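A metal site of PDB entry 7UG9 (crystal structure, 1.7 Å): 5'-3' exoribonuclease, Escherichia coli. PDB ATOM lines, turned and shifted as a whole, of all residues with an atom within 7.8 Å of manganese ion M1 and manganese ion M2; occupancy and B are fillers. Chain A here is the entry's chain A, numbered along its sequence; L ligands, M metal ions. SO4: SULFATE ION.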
ATOM      1  N   HIS A  13     -18.516   9.516  21.728  1.00  0.00           N
ATOM      2  CA  HIS A  13     -19.678   8.644  21.864  1.00  0.00           C
ATOM      3  C   HIS A  13     -19.246   7.237  21.448  1.00  0.00           C
ATOM      4  O   HIS A  13     -19.038   7.000  20.261  1.00  0.00           O
ATOM      5  CB  HIS A  13     -20.838   9.142  21.014  1.00  0.00           C
ATOM      6  CG  HIS A  13     -22.163   8.500  21.345  1.00  0.00           C
ATOM      7  ND1 HIS A  13     -23.346   9.204  21.332  1.00  0.00           N
ATOM      8  CD2 HIS A  13     -22.482   7.224  21.676  1.00  0.00           C
ATOM      9  CE1 HIS A  13     -24.343   8.384  21.626  1.00  0.00           C
ATOM     10  NE2 HIS A  13     -23.855   7.179  21.849  1.00  0.00           N
ATOM     11  N   SER A  14     -19.112   6.337  22.418  1.00  0.00           N
ATOM     12  CA  SER A  14     -18.683   4.968  22.114  1.00  0.00           C
ATOM     13  C   SER A  14     -19.176   4.033  23.205  1.00  0.00           C
ATOM     14  O   SER A  14     -19.480   4.466  24.332  1.00  0.00           O
ATOM     15  CB  SER A  14     -17.152   4.872  22.014  1.00  0.00           C
ATOM     16  OG  SER A  14     -16.555   5.171  23.269  1.00  0.00           O
ATOM     17  N   HIS A  15     -19.248   2.745  22.871  1.00  0.00           N
ATOM     18  CA  HIS A  15     -19.775   1.731  23.785  1.00  0.00           C
ATOM     19  C   HIS A  15     -18.805   0.567  23.941  1.00  0.00           C
ATOM     20  O   HIS A  15     -17.973   0.309  23.069  1.00  0.00           O
ATOM     21  CB  HIS A  15     -21.119   1.183  23.304  1.00  0.00           C
ATOM     22  CG  HIS A  15     -22.187   2.219  23.303  1.00  0.00           C
ATOM     23  ND1 HIS A  15     -23.111   2.307  24.312  1.00  0.00           N
ATOM     24  CD2 HIS A  15     -22.495   3.184  22.414  1.00  0.00           C
ATOM     25  CE1 HIS A  15     -23.929   3.321  24.065  1.00  0.00           C
ATOM     26  NE2 HIS A  15     -23.578   3.869  22.924  1.00  0.00           N
ATOM     27  N   SER A  19     -21.993  -1.959  28.340  1.00  0.00           N
ATOM     28  CA  SER A  19     -23.382  -1.891  27.886  1.00  0.00           C
ATOM     29  C   SER A  19     -23.540  -2.782  26.670  1.00  0.00           C
ATOM     30  O   SER A  19     -23.393  -4.004  26.772  1.00  0.00           O
ATOM     31  CB  SER A  19     -23.839  -0.439  27.639  1.00  0.00           C
ATOM     32  OG  SER A  19     -23.216   0.223  26.566  1.00  0.00           O
ATOM     33  N   ASP A  20     -23.796  -2.217  25.492  1.00  0.00           N
ATOM     34  CA  ASP A  20     -24.105  -3.076  24.347  1.00  0.00           C
ATOM     35  C   ASP A  20     -23.012  -3.059  23.278  1.00  0.00           C
ATOM     36  O   ASP A  20     -23.293  -3.396  22.131  1.00  0.00           O
ATOM     37  CB  ASP A  20     -25.463  -2.717  23.742  1.00  0.00           C
ATOM     38  CG  ASP A  20     -25.562  -1.269  23.286  1.00  0.00           C
ATOM     39  OD1 ASP A  20     -24.651  -0.477  23.606  1.00  0.00           O
ATOM     40  OD2 ASP A  20     -26.549  -0.926  22.609  1.00  0.00           O
ATOM     41  N   THR A  43     -19.319   6.182  26.534  1.00  0.00           N
ATOM     42  CA  THR A  43     -20.657   6.661  26.876  1.00  0.00           C
ATOM     43  C   THR A  43     -21.623   5.462  26.869  1.00  0.00           C
ATOM     44  O   THR A  43     -22.560   5.397  26.080  1.00  0.00           O
ATOM     45  CB  THR A  43     -21.109   7.765  25.913  1.00  0.00           C
ATOM     46  OG1 THR A  43     -21.185   7.285  24.557  1.00  0.00           O
ATOM     47  CG2 THR A  43     -20.144   8.977  25.964  1.00  0.00           C
ATOM     48  N   ASP A  44     -21.384   4.508  27.766  1.00  0.00           N
ATOM     49  CA  ASP A  44     -22.216   3.312  27.847  1.00  0.00           C
ATOM     50  C   ASP A  44     -23.622   3.670  28.348  1.00  0.00           C
ATOM     51  O   ASP A  44     -23.811   4.650  29.053  1.00  0.00           O
ATOM     52  CB  ASP A  44     -21.542   2.281  28.752  1.00  0.00           C
ATOM     53  CG  ASP A  44     -20.507   1.424  28.013  1.00  0.00           C
ATOM     54  OD1 ASP A  44     -20.799   0.961  26.888  1.00  0.00           O
ATOM     55  OD2 ASP A  44     -19.359   1.314  28.499  1.00  0.00           O
ATOM     56  N   HIS A  45     -24.611   2.860  27.943  1.00  0.00           N
ATOM     57  CA  HIS A  45     -25.992   3.066  28.375  1.00  0.00           C
ATOM     58  C   HIS A  45     -26.148   2.925  29.872  1.00  0.00           C
ATOM     59  O   HIS A  45     -25.979   1.831  30.427  1.00  0.00           O
ATOM     60  CB  HIS A  45     -26.923   2.071  27.671  1.00  0.00           C
ATOM     61  CG  HIS A  45     -26.978   2.235  26.190  1.00  0.00           C
ATOM     62  ND1 HIS A  45     -27.604   3.299  25.588  1.00  0.00           N
ATOM     63  CD2 HIS A  45     -26.491   1.464  25.193  1.00  0.00           C
ATOM     64  CE1 HIS A  45     -27.507   3.177  24.274  1.00  0.00           C
ATOM     65  NE2 HIS A  45     -26.811   2.086  24.005  1.00  0.00           N
ATOM     66  N   GLU A  72     -24.423   7.422  28.553  1.00  0.00           N
ATOM     67  CA  GLU A  72     -25.575   7.708  27.702  1.00  0.00           C
ATOM     68  C   GLU A  72     -26.841   7.380  28.470  1.00  0.00           C
ATOM     69  O   GLU A  72     -27.055   6.228  28.851  1.00  0.00           O
ATOM     70  CB  GLU A  72     -25.516   6.925  26.392  1.00  0.00           C
ATOM     71  CG  GLU A  72     -26.588   7.482  25.414  1.00  0.00           C
ATOM     72  CD  GLU A  72     -26.550   6.866  24.049  1.00  0.00           C
ATOM     73  OE1 GLU A  72     -25.803   5.886  23.869  1.00  0.00           O
ATOM     74  OE2 GLU A  72     -27.203   7.425  23.133  1.00  0.00           O
ATOM     75  N   ILE A  73     -27.693   8.396  28.687  1.00  0.00           N
ATOM     76  CA  ILE A  73     -28.894   8.281  29.518  1.00  0.00           C
ATOM     77  C   ILE A  73     -30.117   8.215  28.630  1.00  0.00           C
ATOM     78  O   ILE A  73     -30.248   8.992  27.671  1.00  0.00           O
ATOM     79  CB  ILE A  73     -28.981   9.489  30.478  1.00  0.00           C
ATOM     80  CG1 ILE A  73     -27.766   9.487  31.392  1.00  0.00           C
ATOM     81  CG2 ILE A  73     -30.282   9.443  31.283  1.00  0.00           C
ATOM     82  CD1 ILE A  73     -27.672  10.717  32.319  1.00  0.00           C
ATOM     83  N   SER A  74     -31.024   7.293  28.925  1.00  0.00           N
ATOM     84  CA  SER A  74     -32.239   7.111  28.151  1.00  0.00           C
ATOM     85  C   SER A  74     -33.355   7.944  28.788  1.00  0.00           C
ATOM     86  O   SER A  74     -33.616   7.809  29.984  1.00  0.00           O
ATOM     87  CB  SER A  74     -32.606   5.625  28.118  1.00  0.00           C
ATOM     88  OG  SER A  74     -31.531   4.877  27.564  1.00  0.00           O
ATOM     89  N   GLU A  81     -38.414   8.316  22.707  1.00  0.00           N
ATOM     90  CA  GLU A  81     -37.186   7.969  23.418  1.00  0.00           C
ATOM     91  C   GLU A  81     -36.052   8.874  22.928  1.00  0.00           C
ATOM     92  O   GLU A  81     -35.744   8.906  21.722  1.00  0.00           O
ATOM     93  CB  GLU A  81     -36.821   6.500  23.203  1.00  0.00           C
ATOM     94  CG  GLU A  81     -35.485   6.152  23.852  1.00  0.00           C
ATOM     95  CD  GLU A  81     -35.236   4.655  23.921  1.00  0.00           C
ATOM     96  OE1 GLU A  81     -36.209   3.882  23.797  1.00  0.00           O
ATOM     97  OE2 GLU A  81     -34.064   4.266  24.141  1.00  0.00           O
ATOM     98  N   ILE A  82     -35.443   9.615  23.833  1.00  0.00           N
ATOM     99  CA  ILE A  82     -34.373  10.544  23.507  1.00  0.00           C
ATOM    100  C   ILE A  82     -33.176  10.181  24.352  1.00  0.00           C
ATOM    101  O   ILE A  82     -33.319   9.857  25.539  1.00  0.00           O
ATOM    102  CB  ILE A  82     -34.789  12.022  23.777  1.00  0.00           C
ATOM    103  CG1 ILE A  82     -36.063  12.388  23.006  1.00  0.00           C
ATOM    104  CG2 ILE A  82     -33.671  12.978  23.383  1.00  0.00           C
ATOM    105  CD1 ILE A  82     -35.891  12.361  21.453  1.00  0.00           C
ATOM    106  N   HIS A  83     -31.989  10.221  23.761  1.00  0.00           N
ATOM    107  CA  HIS A  83     -30.764   9.868  24.456  1.00  0.00           C
ATOM    108  C   HIS A  83     -29.951  11.126  24.747  1.00  0.00           C
ATOM    109  O   HIS A  83     -29.711  11.930  23.845  1.00  0.00           O
ATOM    110  CB  HIS A  83     -29.929   8.861  23.637  1.00  0.00           C
ATOM    111  CG  HIS A  83     -30.573   7.507  23.512  1.00  0.00           C
ATOM    112  ND1 HIS A  83     -30.142   6.543  22.624  1.00  0.00           N
ATOM    113  CD2 HIS A  83     -31.650   6.971  24.148  1.00  0.00           C
ATOM    114  CE1 HIS A  83     -30.902   5.458  22.735  1.00  0.00           C
ATOM    115  NE2 HIS A  83     -31.817   5.696  23.665  1.00  0.00           N
ATOM    116  N   ILE A  84     -29.532  11.273  25.993  1.00  0.00           N
ATOM    117  CA  ILE A  84     -28.717  12.387  26.452  1.00  0.00           C
ATOM    118  C   ILE A  84     -27.401  11.822  26.927  1.00  0.00           C
ATOM    119  O   ILE A  84     -27.384  10.892  27.742  1.00  0.00           O
ATOM    120  CB  ILE A  84     -29.401  13.176  27.594  1.00  0.00           C
ATOM    121  CG1 ILE A  84     -30.834  13.581  27.215  1.00  0.00           C
ATOM    122  CG2 ILE A  84     -28.569  14.363  28.031  1.00  0.00           C
ATOM    123  CD1 ILE A  84     -30.884  14.599  26.108  1.00  0.00           C
ATOM    124  N   VAL A  85     -26.307  12.340  26.400  1.00  0.00           N
ATOM    125  CA  VAL A  85     -24.974  11.899  26.778  1.00  0.00           C
ATOM    126  C   VAL A  85     -24.459  12.898  27.813  1.00  0.00           C
ATOM    127  O   VAL A  85     -24.659  14.099  27.660  1.00  0.00           O
ATOM    128  CB  VAL A  85     -24.056  11.837  25.556  1.00  0.00           C
ATOM    129  CG1 VAL A  85     -22.589  11.744  25.969  1.00  0.00           C
ATOM    130  CG2 VAL A  85     -24.436  10.632  24.682  1.00  0.00           C
ATOM    131  N   ALA A 197     -27.917  13.551  22.015  1.00  0.00           N
ATOM    132  CA  ALA A 197     -27.254  12.583  21.150  1.00  0.00           C
ATOM    133  C   ALA A 197     -28.005  12.379  19.850  1.00  0.00           C
ATOM    134  O   ALA A 197     -29.239  12.453  19.802  1.00  0.00           O
ATOM    135  CB  ALA A 197     -27.127  11.253  21.870  1.00  0.00           C
ATOM    136  N   HIS A 198     -27.235  12.063  18.781  1.00  0.00           N
ATOM    137  CA  HIS A 198     -27.654  11.681  17.431  1.00  0.00           C
ATOM    138  C   HIS A 198     -29.028  12.240  17.086  1.00  0.00           C
ATOM    139  O   HIS A 198     -30.001  11.491  16.929  1.00  0.00           O
ATOM    140  CB  HIS A 198     -27.613  10.149  17.245  1.00  0.00           C
ATOM    141  CG  HIS A 198     -28.112   9.345  18.414  1.00  0.00           C
ATOM    142  ND1 HIS A 198     -29.424   9.335  18.818  1.00  0.00           N
ATOM    143  CD2 HIS A 198     -27.457   8.480  19.227  1.00  0.00           C
ATOM    144  CE1 HIS A 198     -29.562   8.533  19.856  1.00  0.00           C
ATOM    145  NE2 HIS A 198     -28.382   7.987  20.124  1.00  0.00           N
ATOM    146  N   ARG A 201     -31.286  10.770  14.236  1.00  0.00           N
ATOM    147  CA  ARG A 201     -31.852   9.420  14.344  1.00  0.00           C
ATOM    148  C   ARG A 201     -33.258   9.398  14.886  1.00  0.00           C
ATOM    149  O   ARG A 201     -33.924   8.359  14.809  1.00  0.00           O
ATOM    150  CB  ARG A 201     -30.970   8.530  15.225  1.00  0.00           C
ATOM    151  CG  ARG A 201     -29.928   7.788  14.433  1.00  0.00           C
ATOM    152  CD  ARG A 201     -29.249   6.660  15.209  1.00  0.00           C
ATOM    153  NE  ARG A 201     -29.969   6.173  16.380  1.00  0.00           N
ATOM    154  CZ  ARG A 201     -29.377   5.508  17.356  1.00  0.00           C
ATOM    155  NH1 ARG A 201     -28.088   5.255  17.328  1.00  0.00           N
ATOM    156  NH2 ARG A 201     -30.097   5.102  18.411  1.00  0.00           N
ATOM    157  N   TYR A 202     -33.761  10.503  15.445  1.00  0.00           N
ATOM    158  CA  TYR A 202     -35.092  10.446  15.999  1.00  0.00           C
ATOM    159  C   TYR A 202     -36.146  10.582  14.911  1.00  0.00           C
ATOM    160  O   TYR A 202     -37.341  10.439  15.199  1.00  0.00           O
ATOM    161  CB  TYR A 202     -35.251  11.539  17.062  1.00  0.00           C
ATOM    162  CG  TYR A 202     -34.203  11.444  18.167  1.00  0.00           C
ATOM    163  CD1 TYR A 202     -33.940  10.237  18.827  1.00  0.00           C
ATOM    164  CD2 TYR A 202     -33.427  12.551  18.486  1.00  0.00           C
ATOM    165  CE1 TYR A 202     -32.981  10.155  19.831  1.00  0.00           C
ATOM    166  CE2 TYR A 202     -32.454  12.479  19.473  1.00  0.00           C
ATOM    167  CZ  TYR A 202     -32.240  11.274  20.134  1.00  0.00           C
ATOM    168  OH  TYR A 202     -31.281  11.209  21.114  1.00  0.00           O
ATOM    169  N   GLU A 225     -24.872  16.603  19.514  1.00  0.00           N
ATOM    170  CA  GLU A 225     -24.014  15.906  18.569  1.00  0.00           C
ATOM    171  C   GLU A 225     -24.328  16.401  17.171  1.00  0.00           C
ATOM    172  O   GLU A 225     -25.487  16.409  16.736  1.00  0.00           O
ATOM    173  CB  GLU A 225     -24.212  14.390  18.673  1.00  0.00           C
ATOM    174  CG  GLU A 225     -23.628  13.860  19.950  1.00  0.00           C
ATOM    175  CD  GLU A 225     -23.707  12.348  20.081  1.00  0.00           C
ATOM    176  OE1 GLU A 225     -24.354  11.673  19.246  1.00  0.00           O
ATOM    177  OE2 GLU A 225     -23.098  11.838  21.043  1.00  0.00           O
ATOM    178  N   SER A 254     -18.805   8.632  17.122  1.00  0.00           N
ATOM    179  CA  SER A 254     -19.091   7.567  16.176  1.00  0.00           C
ATOM    180  C   SER A 254     -20.266   6.715  16.604  1.00  0.00           C
ATOM    181  O   SER A 254     -20.877   6.052  15.753  1.00  0.00           O
ATOM    182  CB  SER A 254     -17.870   6.661  15.999  1.00  0.00           C
ATOM    183  OG  SER A 254     -17.441   6.127  17.248  1.00  0.00           O
ATOM    184  N   ASP A 255     -20.577   6.685  17.909  1.00  0.00           N
ATOM    185  CA  ASP A 255     -21.525   5.727  18.460  1.00  0.00           C
ATOM    186  C   ASP A 255     -21.074   4.307  18.170  1.00  0.00           C
ATOM    187  O   ASP A 255     -21.869   3.426  17.861  1.00  0.00           O
ATOM    188  CB  ASP A 255     -22.928   5.960  17.901  1.00  0.00           C
ATOM    189  CG  ASP A 255     -24.011   5.434  18.788  1.00  0.00           C
ATOM    190  OD1 ASP A 255     -23.719   4.926  19.884  1.00  0.00           O
ATOM    191  OD2 ASP A 255     -25.184   5.485  18.358  1.00  0.00           O
ATOM    192  N   PHE A 256     -19.765   4.105  18.238  1.00  0.00           N
ATOM    193  CA  PHE A 256     -19.194   2.788  17.959  1.00  0.00           C
ATOM    194  C   PHE A 256     -19.707   1.732  18.929  1.00  0.00           C
ATOM    195  O   PHE A 256     -19.635   1.900  20.141  1.00  0.00           O
ATOM    196  CB  PHE A 256     -17.674   2.891  18.045  1.00  0.00           C
ATOM    197  CG  PHE A 256     -16.970   1.589  17.837  1.00  0.00           C
ATOM    198  CD1 PHE A 256     -16.734   0.726  18.894  1.00  0.00           C
ATOM    199  CD2 PHE A 256     -16.546   1.233  16.568  1.00  0.00           C
ATOM    200  CE1 PHE A 256     -16.065  -0.488  18.686  1.00  0.00           C
ATOM    201  CE2 PHE A 256     -15.864   0.058  16.362  1.00  0.00           C
ATOM    202  CZ  PHE A 256     -15.650  -0.813  17.426  1.00  0.00           C
ATOM    203  N   HIS A 257     -20.167   0.609  18.368  1.00  0.00           N
ATOM    204  CA  HIS A 257     -20.503  -0.591  19.141  1.00  0.00           C
ATOM    205  C   HIS A 257     -19.607  -1.775  18.796  1.00  0.00           C
ATOM    206  O   HIS A 257     -19.146  -2.473  19.688  1.00  0.00           O
ATOM    207  CB  HIS A 257     -21.958  -1.012  18.895  1.00  0.00           C
ATOM    208  CG  HIS A 257     -22.962  -0.126  19.544  1.00  0.00           C
ATOM    209  ND1 HIS A 257     -23.173   1.177  19.145  1.00  0.00           N
ATOM    210  CD2 HIS A 257     -23.870  -0.363  20.534  1.00  0.00           C
ATOM    211  CE1 HIS A 257     -24.134   1.711  19.867  1.00  0.00           C
ATOM    212  NE2 HIS A 257     -24.561   0.808  20.737  1.00  0.00           N
HETATM  213  S   SO4 L   1     -27.227   4.084  20.656  1.00  0.00           S
HETATM  214  O1  SO4 L   1     -28.610   4.215  21.109  1.00  0.00           O
HETATM  215  O2  SO4 L   1     -26.644   5.414  20.850  1.00  0.00           O
HETATM  216  O3  SO4 L   1     -26.425   3.141  21.415  1.00  0.00           O
HETATM  217  O4  SO4 L   1     -27.191   3.702  19.246  1.00  0.00           O
HETATM  218 MN    MN M   1     -28.264   6.532  21.647  1.00  0.00          MN
HETATM  219 MN    MN M   2     -24.858   5.262  21.928  1.00  0.00          MN
HETATM  220 MN    MN M   3     -26.241   1.156  22.070  1.00  0.00          MN
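The nearest printed residue that does not touch manganese ion M2 is His 45 (4.1 Å).
NH2 of Arg 201 touches manganese ion M1, 3.98 Å away. Within 4 Å of manganese ion M1: Glu 72, His 83, His 198 and Arg 201. The nearest printed residue that does not touch manganese ion M1 is His 45 (4.3 Å).
Manganese ion M2 is bound by O2 of the ligand (2.1 Å), NE2 of His 15 (2.1 Å), NE2 of His 13 (2.2 Å), OE1 of Glu 72 (2.2 Å), OD1 of Asp 255 (2.4 Å) and O3 of the ligand (2.7 Å). Manganese ion M2 has six donor atoms within binding distance.
Manganese ion M1 is bound by OE2 of Glu 72, at 2.0 Å. NE2 of His 198 is bound to manganese ion M1 (2.1 Å). Manganese ion M1 is bound by ND1 of His 83, at 2.1 Å. An oxygen (O2) of the ligand is bound to manganese ion M1. O1 of the ligand binds manganese ion M1 (2.4 Å).
N of Glu 72 lies within hydrogen-bond range of O of Asp 44 (2.9 Å). The side-chain hydroxyl (OH) of Tyr 202 sits close to a ring nitrogen (ND1) of His 198, at 3.5 Å. N of His 198 sits at hydrogen-bond distance from OE1 of Glu 225 (2.9 Å). N of Ala 197 sits at hydrogen-bond distance from O of His 83, 3.0 Å away. The side-chain carboxylate of Glu 81 is in hydrogen-bond range of a ring nitrogen (NE2) of His 83 (2.7 Å). ND1 of His 15 lies within hydrogen-bond range of OG of Ser 19 (3.1 Å). The side-chain carboxylate (OD2) of Asp 255 lies within salt-bridge range of the guanidinium group (NH1) of Arg 201 (3.1 Å). ND1 of His 257 lies within hydrogen-bond range of O of Asp 255.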
